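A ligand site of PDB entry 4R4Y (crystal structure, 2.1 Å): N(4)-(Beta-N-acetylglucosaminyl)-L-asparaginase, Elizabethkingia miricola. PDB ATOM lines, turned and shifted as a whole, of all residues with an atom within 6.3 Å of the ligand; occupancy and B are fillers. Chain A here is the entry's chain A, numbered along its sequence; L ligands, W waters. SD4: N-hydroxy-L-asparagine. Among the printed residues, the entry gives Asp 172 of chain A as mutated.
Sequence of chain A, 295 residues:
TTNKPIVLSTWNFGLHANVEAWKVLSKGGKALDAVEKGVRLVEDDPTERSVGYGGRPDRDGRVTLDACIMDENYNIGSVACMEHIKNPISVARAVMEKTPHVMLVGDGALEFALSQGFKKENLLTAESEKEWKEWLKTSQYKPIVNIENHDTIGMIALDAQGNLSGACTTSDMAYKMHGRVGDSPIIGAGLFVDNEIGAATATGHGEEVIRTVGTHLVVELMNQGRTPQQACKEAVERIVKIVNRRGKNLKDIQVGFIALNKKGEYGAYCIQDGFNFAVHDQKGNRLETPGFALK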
ATOM      1  N   TRP A  11      24.365 -11.106  24.431  1.00  0.00           N
ATOM      2  CA  TRP A  11      25.515 -11.946  24.261  1.00  0.00           C
ATOM      3  C   TRP A  11      26.034 -12.559  25.527  1.00  0.00           C
ATOM      4  O   TRP A  11      25.527 -12.274  26.581  1.00  0.00           O
ATOM      5  CB  TRP A  11      26.700 -11.218  23.575  1.00  0.00           C
ATOM      6  CG  TRP A  11      26.372 -10.536  22.280  1.00  0.00           C
ATOM      7  CD1 TRP A  11      26.268  -9.189  22.045  1.00  0.00           C
ATOM      8  CD2 TRP A  11      26.083 -11.172  21.048  1.00  0.00           C
ATOM      9  NE1 TRP A  11      25.961  -8.952  20.732  1.00  0.00           N
ATOM     10  CE2 TRP A  11      25.857 -10.153  20.096  1.00  0.00           C
ATOM     11  CE3 TRP A  11      26.001 -12.499  20.649  1.00  0.00           C
ATOM     12  CZ2 TRP A  11      25.552 -10.426  18.763  1.00  0.00           C
ATOM     13  CZ3 TRP A  11      25.750 -12.768  19.280  1.00  0.00           C
ATOM     14  CH2 TRP A  11      25.498 -11.738  18.384  1.00  0.00           C
ATOM     15  N   ARG A  56      38.285  -3.134  20.113  1.00  0.00           N
ATOM     16  CA  ARG A  56      38.328  -3.068  18.651  1.00  0.00           C
ATOM     17  C   ARG A  56      38.858  -1.662  18.290  1.00  0.00           C
ATOM     18  O   ARG A  56      38.449  -0.680  18.884  1.00  0.00           O
ATOM     19  CB  ARG A  56      36.947  -3.335  18.020  1.00  0.00           C
ATOM     20  CG  ARG A  56      36.184  -4.590  18.524  1.00  0.00           C
ATOM     21  CD  ARG A  56      36.777  -5.855  17.950  1.00  0.00           C
ATOM     22  NE  ARG A  56      36.306  -7.115  18.557  1.00  0.00           N
ATOM     23  CZ  ARG A  56      35.076  -7.635  18.418  1.00  0.00           C
ATOM     24  NH1 ARG A  56      34.108  -7.000  17.753  1.00  0.00           N
ATOM     25  NH2 ARG A  56      34.823  -8.815  18.986  1.00  0.00           N
ATOM     26  N   ASP A  66      31.474   4.007  22.115  1.00  0.00           N
ATOM     27  CA  ASP A  66      30.129   4.523  22.064  1.00  0.00           C
ATOM     28  C   ASP A  66      29.388   3.871  23.216  1.00  0.00           C
ATOM     29  O   ASP A  66      29.435   2.648  23.384  1.00  0.00           O
ATOM     30  CB  ASP A  66      29.439   4.063  20.796  1.00  0.00           C
ATOM     31  CG  ASP A  66      30.081   4.599  19.565  1.00  0.00           C
ATOM     32  OD1 ASP A  66      30.869   5.542  19.729  1.00  0.00           O
ATOM     33  OD2 ASP A  66      29.834   4.062  18.453  1.00  0.00           O
ATOM     34  N   ILE A 144      31.029  -7.474  10.601  1.00  0.00           N
ATOM     35  CA  ILE A 144      30.307  -8.680  10.941  1.00  0.00           C
ATOM     36  C   ILE A 144      29.891  -8.675  12.379  1.00  0.00           C
ATOM     37  O   ILE A 144      30.634  -8.237  13.220  1.00  0.00           O
ATOM     38  CB  ILE A 144      31.164  -9.919  10.834  1.00  0.00           C
ATOM     39  CG1 ILE A 144      31.756  -9.999   9.432  1.00  0.00           C
ATOM     40  CG2 ILE A 144      30.346 -11.132  11.258  1.00  0.00           C
ATOM     41  CD1 ILE A 144      32.240 -11.374   9.013  1.00  0.00           C
ATOM     42  N   VAL A 145      28.699  -9.207  12.662  1.00  0.00           N
ATOM     43  CA  VAL A 145      28.200  -9.266  14.025  1.00  0.00           C
ATOM     44  C   VAL A 145      27.518 -10.594  14.223  1.00  0.00           C
ATOM     45  O   VAL A 145      26.418 -10.825  13.743  1.00  0.00           O
ATOM     46  CB  VAL A 145      27.243  -8.126  14.349  1.00  0.00           C
ATOM     47  CG1 VAL A 145      26.675  -8.298  15.756  1.00  0.00           C
ATOM     48  CG2 VAL A 145      27.960  -6.792  14.198  1.00  0.00           C
ATOM     49  N   ASN A 149      31.960 -12.848  16.590  1.00  0.00           N
ATOM     50  CA  ASN A 149      32.372 -11.461  16.369  1.00  0.00           C
ATOM     51  C   ASN A 149      31.354 -10.505  16.918  1.00  0.00           C
ATOM     52  O   ASN A 149      30.501 -10.146  16.195  1.00  0.00           O
ATOM     53  CB  ASN A 149      32.382 -11.167  14.890  1.00  0.00           C
ATOM     54  CG  ASN A 149      33.670 -11.498  14.241  1.00  0.00           C
ATOM     55  OD1 ASN A 149      34.423 -10.617  13.881  1.00  0.00           O
ATOM     56  ND2 ASN A 149      33.924 -12.754  14.075  1.00  0.00           N
ATOM     57  N   HIS A 150      31.454 -10.057  18.170  1.00  0.00           N
ATOM     58  CA  HIS A 150      30.626  -8.974  18.679  1.00  0.00           C
ATOM     59  C   HIS A 150      31.305  -8.348  19.881  1.00  0.00           C
ATOM     60  O   HIS A 150      32.316  -8.874  20.423  1.00  0.00           O
ATOM     61  CB  HIS A 150      29.293  -9.467  19.120  1.00  0.00           C
ATOM     62  CG  HIS A 150      29.367 -10.535  20.142  1.00  0.00           C
ATOM     63  ND1 HIS A 150      29.423 -11.869  19.812  1.00  0.00           N
ATOM     64  CD2 HIS A 150      29.445 -10.467  21.485  1.00  0.00           C
ATOM     65  CE1 HIS A 150      29.515 -12.589  20.919  1.00  0.00           C
ATOM     66  NE2 HIS A 150      29.548 -11.765  21.951  1.00  0.00           N
ATOM     67  N   ASP A 151      30.786  -7.208  20.287  1.00  0.00           N
ATOM     68  CA  ASP A 151      31.392  -6.437  21.356  1.00  0.00           C
ATOM     69  C   ASP A 151      30.399  -5.556  22.111  1.00  0.00           C
ATOM     70  O   ASP A 151      30.744  -4.483  22.565  1.00  0.00           O
ATOM     71  CB  ASP A 151      32.512  -5.566  20.810  1.00  0.00           C
ATOM     72  CG  ASP A 151      33.396  -5.004  21.875  1.00  0.00           C
ATOM     73  OD1 ASP A 151      33.835  -5.784  22.748  1.00  0.00           O
ATOM     74  OD2 ASP A 151      33.668  -3.790  21.850  1.00  0.00           O
ATOM     75  N   THR A 152      29.179  -6.013  22.296  1.00  0.00           N
ATOM     76  CA  THR A 152      28.161  -5.152  22.860  1.00  0.00           C
ATOM     77  C   THR A 152      27.665  -5.710  24.146  1.00  0.00           C
ATOM     78  O   THR A 152      27.484  -6.909  24.266  1.00  0.00           O
ATOM     79  CB  THR A 152      26.983  -5.020  21.890  1.00  0.00           C
ATOM     80  OG1 THR A 152      27.470  -4.458  20.677  1.00  0.00           O
ATOM     81  CG2 THR A 152      25.879  -4.102  22.396  1.00  0.00           C
ATOM     82  N   THR A 170      29.763  -0.332  23.269  1.00  0.00           N
ATOM     83  CA  THR A 170      30.613  -1.164  22.407  1.00  0.00           C
ATOM     84  C   THR A 170      31.828  -0.394  22.002  1.00  0.00           C
ATOM     85  O   THR A 170      31.898   0.812  22.197  1.00  0.00           O
ATOM     86  CB  THR A 170      29.873  -1.601  21.121  1.00  0.00           C
ATOM     87  OG1 THR A 170      30.620  -2.646  20.455  1.00  0.00           O
ATOM     88  CG2 THR A 170      29.642  -0.382  20.166  1.00  0.00           C
ATOM     89  N   SER A 171      32.826  -1.085  21.445  1.00  0.00           N
ATOM     90  CA  SER A 171      33.864  -0.436  20.658  1.00  0.00           C
ATOM     91  C   SER A 171      33.648  -0.738  19.177  1.00  0.00           C
ATOM     92  O   SER A 171      34.418  -0.274  18.309  1.00  0.00           O
ATOM     93  CB  SER A 171      35.245  -0.927  21.105  1.00  0.00           C
ATOM     94  OG  SER A 171      35.556  -2.182  20.579  1.00  0.00           O
ATOM     95  N   ASP A 172      32.651  -1.564  18.869  1.00  0.00           N
ATOM     96  CA  ASP A 172      32.433  -1.954  17.444  1.00  0.00           C
ATOM     97  C   ASP A 172      32.149  -0.752  16.574  1.00  0.00           C
ATOM     98  O   ASP A 172      31.774   0.301  17.113  1.00  0.00           O
ATOM     99  CB  ASP A 172      31.320  -2.957  17.294  1.00  0.00           C
ATOM    100  CG  ASP A 172      31.815  -4.378  17.470  1.00  0.00           C
ATOM    101  OD1 ASP A 172      33.036  -4.609  17.216  1.00  0.00           O
ATOM    102  OD2 ASP A 172      31.019  -5.259  17.888  1.00  0.00           O
ATOM    103  N   MET A 173      32.321  -0.845  15.249  1.00  0.00           N
ATOM    104  CA  MET A 173      32.883  -1.979  14.511  1.00  0.00           C
ATOM    105  C   MET A 173      34.378  -1.822  14.325  1.00  0.00           C
ATOM    106  O   MET A 173      34.850  -0.759  14.022  1.00  0.00           O
ATOM    107  CB  MET A 173      32.306  -2.005  13.093  1.00  0.00           C
ATOM    108  CG  MET A 173      30.790  -2.205  12.956  1.00  0.00           C
ATOM    109  SD  MET A 173      30.132  -3.729  13.636  1.00  0.00           S
ATOM    110  CE  MET A 173      31.277  -4.880  12.891  1.00  0.00           C
ATOM    111  N   LYS A 176      36.154   0.562  11.487  1.00  0.00           N
ATOM    112  CA  LYS A 176      35.285   1.643  11.079  1.00  0.00           C
ATOM    113  C   LYS A 176      36.113   2.849  10.735  1.00  0.00           C
ATOM    114  O   LYS A 176      37.208   2.970  11.202  1.00  0.00           O
ATOM    115  CB  LYS A 176      34.339   2.008  12.215  1.00  0.00           C
ATOM    116  CG  LYS A 176      35.035   2.492  13.443  1.00  0.00           C
ATOM    117  CD  LYS A 176      34.122   2.422  14.644  1.00  0.00           C
ATOM    118  CE  LYS A 176      34.914   2.673  15.902  1.00  0.00           C
ATOM    119  NZ  LYS A 176      34.050   2.482  17.105  1.00  0.00           N
ATOM    120  N   ARG A 180      33.435   7.401  13.177  1.00  0.00           N
ATOM    121  CA  ARG A 180      32.134   6.693  12.903  1.00  0.00           C
ATOM    122  C   ARG A 180      31.385   6.481  14.230  1.00  0.00           C
ATOM    123  O   ARG A 180      31.951   5.971  15.225  1.00  0.00           O
ATOM    124  CB  ARG A 180      32.389   5.335  12.213  1.00  0.00           C
ATOM    125  CG  ARG A 180      31.168   4.501  11.817  1.00  0.00           C
ATOM    126  CD  ARG A 180      30.604   3.733  12.999  1.00  0.00           C
ATOM    127  NE  ARG A 180      29.589   2.737  12.656  1.00  0.00           N
ATOM    128  CZ  ARG A 180      29.249   1.768  13.476  1.00  0.00           C
ATOM    129  NH1 ARG A 180      29.880   1.640  14.669  1.00  0.00           N
ATOM    130  NH2 ARG A 180      28.343   0.860  13.094  1.00  0.00           N
ATOM    131  N   VAL A 181      30.091   6.760  14.204  1.00  0.00           N
ATOM    132  CA  VAL A 181      29.213   6.471  15.356  1.00  0.00           C
ATOM    133  C   VAL A 181      28.169   5.443  14.988  1.00  0.00           C
ATOM    134  O   VAL A 181      27.432   5.616  13.998  1.00  0.00           O
ATOM    135  CB  VAL A 181      28.529   7.723  15.866  1.00  0.00           C
ATOM    136  CG1 VAL A 181      27.485   7.408  16.946  1.00  0.00           C
ATOM    137  CG2 VAL A 181      29.581   8.662  16.411  1.00  0.00           C
ATOM    138  N   GLY A 182      28.072   4.423  15.834  1.00  0.00           N
ATOM    139  CA  GLY A 182      27.075   3.421  15.692  1.00  0.00           C
ATOM    140  C   GLY A 182      25.798   3.763  16.425  1.00  0.00           C
ATOM    141  O   GLY A 182      25.567   4.926  16.794  1.00  0.00           O
ATOM    142  N   ASP A 183      24.938   2.759  16.545  1.00  0.00           N
ATOM    143  CA  ASP A 183      23.683   2.909  17.280  1.00  0.00           C
ATOM    144  C   ASP A 183      23.834   2.954  18.795  1.00  0.00           C
ATOM    145  O   ASP A 183      23.000   3.524  19.469  1.00  0.00           O
ATOM    146  CB  ASP A 183      22.739   1.737  16.930  1.00  0.00           C
ATOM    147  CG  ASP A 183      23.306   0.361  17.339  1.00  0.00           C
ATOM    148  OD1 ASP A 183      24.410  -0.003  16.944  1.00  0.00           O
ATOM    149  OD2 ASP A 183      22.603  -0.351  18.032  1.00  0.00           O
ATOM    150  N   SER A 184      24.875   2.318  19.309  1.00  0.00           N
ATOM    151  CA  SER A 184      25.068   2.088  20.731  1.00  0.00           C
ATOM    152  C   SER A 184      24.902   3.304  21.643  1.00  0.00           C
ATOM    153  O   SER A 184      24.363   3.163  22.738  1.00  0.00           O
ATOM    154  CB  SER A 184      26.418   1.415  21.006  1.00  0.00           C
ATOM    155  OG  SER A 184      26.652   0.304  20.140  1.00  0.00           O
ATOM    156  N   ALA A 202      19.694  -3.362  21.666  1.00  0.00           N
ATOM    157  CA  ALA A 202      19.925  -3.918  20.368  1.00  0.00           C
ATOM    158  C   ALA A 202      21.358  -4.180  20.193  1.00  0.00           C
ATOM    159  O   ALA A 202      22.181  -3.637  20.908  1.00  0.00           O
ATOM    160  CB  ALA A 202      19.478  -2.960  19.240  1.00  0.00           C
ATOM    161  N   THR A 203      21.634  -4.971  19.167  1.00  0.00           N
ATOM    162  CA  THR A 203      22.993  -5.315  18.740  1.00  0.00           C
ATOM    163  C   THR A 203      22.833  -5.654  17.240  1.00  0.00           C
ATOM    164  O   THR A 203      21.753  -5.995  16.774  1.00  0.00           O
ATOM    165  CB  THR A 203      23.576  -6.475  19.567  1.00  0.00           C
ATOM    166  OG1 THR A 203      24.937  -6.725  19.148  1.00  0.00           O
ATOM    167  CG2 THR A 203      22.764  -7.723  19.442  1.00  0.00           C
ATOM    168  N   GLY A 204      23.920  -5.487  16.506  1.00  0.00           N
ATOM    169  CA  GLY A 204      23.927  -5.744  15.088  1.00  0.00           C
ATOM    170  C   GLY A 204      24.537  -4.590  14.371  1.00  0.00           C
ATOM    171  O   GLY A 204      25.273  -3.763  14.941  1.00  0.00           O
ATOM    172  N   HIS A 205      24.233  -4.489  13.089  1.00  0.00           N
ATOM    173  CA  HIS A 205      24.821  -3.459  12.330  1.00  0.00           C
ATOM    174  C   HIS A 205      24.141  -2.158  12.648  1.00  0.00           C
ATOM    175  O   HIS A 205      22.977  -1.972  12.343  1.00  0.00           O
ATOM    176  CB  HIS A 205      24.663  -3.758  10.858  1.00  0.00           C
ATOM    177  CG  HIS A 205      25.552  -4.857  10.420  1.00  0.00           C
ATOM    178  ND1 HIS A 205      25.229  -6.182  10.599  1.00  0.00           N
ATOM    179  CD2 HIS A 205      26.755  -4.829   9.802  1.00  0.00           C
ATOM    180  CE1 HIS A 205      26.194  -6.928  10.102  1.00  0.00           C
ATOM    181  NE2 HIS A 205      27.140  -6.126   9.641  1.00  0.00           N
ATOM    182  N   GLY A 206      24.913  -1.271  13.265  1.00  0.00           N
ATOM    183  CA  GLY A 206      24.395  -0.104  13.910  1.00  0.00           C
ATOM    184  C   GLY A 206      23.678   0.833  12.931  1.00  0.00           C
ATOM    185  O   GLY A 206      22.616   1.352  13.252  1.00  0.00           O
ATOM    186  N   GLU A 207      24.269   1.035  11.767  1.00  0.00           N
ATOM    187  CA  GLU A 207      23.656   1.833  10.739  1.00  0.00           C
ATOM    188  C   GLU A 207      22.162   1.433  10.532  1.00  0.00           C
ATOM    189  O   GLU A 207      21.321   2.290  10.258  1.00  0.00           O
ATOM    190  CB  GLU A 207      24.427   1.620   9.407  1.00  0.00           C
ATOM    191  CG  GLU A 207      25.748   2.345   9.297  1.00  0.00           C
ATOM    192  CD  GLU A 207      26.870   1.854  10.212  1.00  0.00           C
ATOM    193  OE1 GLU A 207      26.877   0.720  10.718  1.00  0.00           O
ATOM    194  OE2 GLU A 207      27.790   2.666  10.460  1.00  0.00           O
ATOM    195  N   VAL A 209      20.176  -0.177  12.709  1.00  0.00           N
ATOM    196  CA  VAL A 209      19.457   0.205  13.898  1.00  0.00           C
ATOM    197  C   VAL A 209      19.181   1.731  13.912  1.00  0.00           C
ATOM    198  O   VAL A 209      18.055   2.143  14.253  1.00  0.00           O
ATOM    199  CB  VAL A 209      20.156  -0.181  15.181  1.00  0.00           C
ATOM    200  CG1 VAL A 209      19.313   0.286  16.338  1.00  0.00           C
ATOM    201  CG2 VAL A 209      20.282  -1.697  15.280  1.00  0.00           C
HETATM  202  C   SD4 L   1      27.725  -1.053  16.144  1.00  0.00           C
HETATM  203  N   SD4 L   1      25.859  -2.143  17.185  1.00  0.00           N
HETATM  204  O   SD4 L   1      28.663  -0.355  16.503  1.00  0.00           O
HETATM  205  CA  SD4 L   1      27.312  -2.112  17.138  1.00  0.00           C
HETATM  206  CB  SD4 L   1      27.884  -3.425  16.677  1.00  0.00           C
HETATM  207  CG  SD4 L   1      27.506  -4.514  17.591  1.00  0.00           C
HETATM  208  OAD SD4 L   1      28.272  -6.298  18.820  1.00  0.00           O
HETATM  209  OD1 SD4 L   1      26.382  -4.758  17.980  1.00  0.00           O
HETATM  210  ND2 SD4 L   1      28.523  -5.243  17.975  1.00  0.00           N
HETATM  211  OXT SD4 L   1      27.109  -0.861  15.036  1.00  0.00           O
HETATM  212  O   HOH W   1      23.880  -2.190  19.398  1.00  0.00           O
HETATM  213  O   HOH W   2      27.901   1.664  18.308  1.00  0.00           O
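Val 145 touches the ligand (CG1 to OAD, 3.99 Å). His 150 touches the ligand. Thr 170 touches the ligand. SD of Met 173 touches CB of the ligand, at 3.8 Å. OG of Ser 184 touches CA of the ligand, 3.9 Å away.
OD2 of Asp 172 sits at hydrogen-bond distance from ND2 of the ligand (2.5 Å). The side-chain carboxylate of Asp 183 lies within salt-bridge range of a nitrogen (N) of the ligand (2.6 Å). OD1 of the ligand lies within hydrogen-bond range of OG1 of Thr 203, 2.7 Å away. OAD of the ligand sits at hydrogen-bond distance from OG1 of Thr 152 (2.7 Å). The backbone NH of Gly 204 sits at hydrogen-bond distance from an oxygen (OD1) of the ligand, at 3.0 Å. The backbone carbonyl oxygen (O) of Gly 204 lies within hydrogen-bond range of a nitrogen (N) of the ligand. OXT of the ligand is in hydrogen-bond range of N of Gly 206, 2.9 Å away. NH2 of Arg 180 is in salt-bridge range of OXT of the ligand, at 2.9 Å. The backbone NH (N) of Asp 151 sits at hydrogen-bond distance from an oxygen (OAD) of the ligand, 3.0 Å away.
The backbone carbonyl oxygen (O) of Asp 172 lies within hydrogen-bond range of the guanidinium group (NH1) of Arg 180 (3.4 Å). OD2 of Asp 172 is in hydrogen-bond range of N of Asp 151, at 3.1 Å. OG1 of Thr 170 sits at hydrogen-bond distance from N of Asp 172 (2.8 Å). The guanidinium group of Arg 56 lies within salt-bridge range of the side-chain carboxylate of Asp 172 (2.7 Å). The backbone carbonyl oxygen of Asp 172 sits at hydrogen-bond distance from the side-chain amino group of Lys 176. The guanidinium group of Arg 180 is in salt-bridge range of the side-chain carboxylate of Glu 207, at 2.8 Å. OG of Ser 171 sits at hydrogen-bond distance from OD2 of Asp 151, 2.8 Å away. O of Asp 66 lies within hydrogen-bond range of N of Thr 170.
Water W2 lies within hydrogen-bond range of the side-chain hydroxyl of Ser 184 (2.6 Å), an oxygen (O) of the ligand (2.8 Å) and the side-chain carboxylate of Asp 66 (3.1 Å). Water W1 lies within hydrogen-bond range of the side-chain carboxylate of Asp 183, the backbone carbonyl oxygen of Ala 202 and a nitrogen (N) of the ligand.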
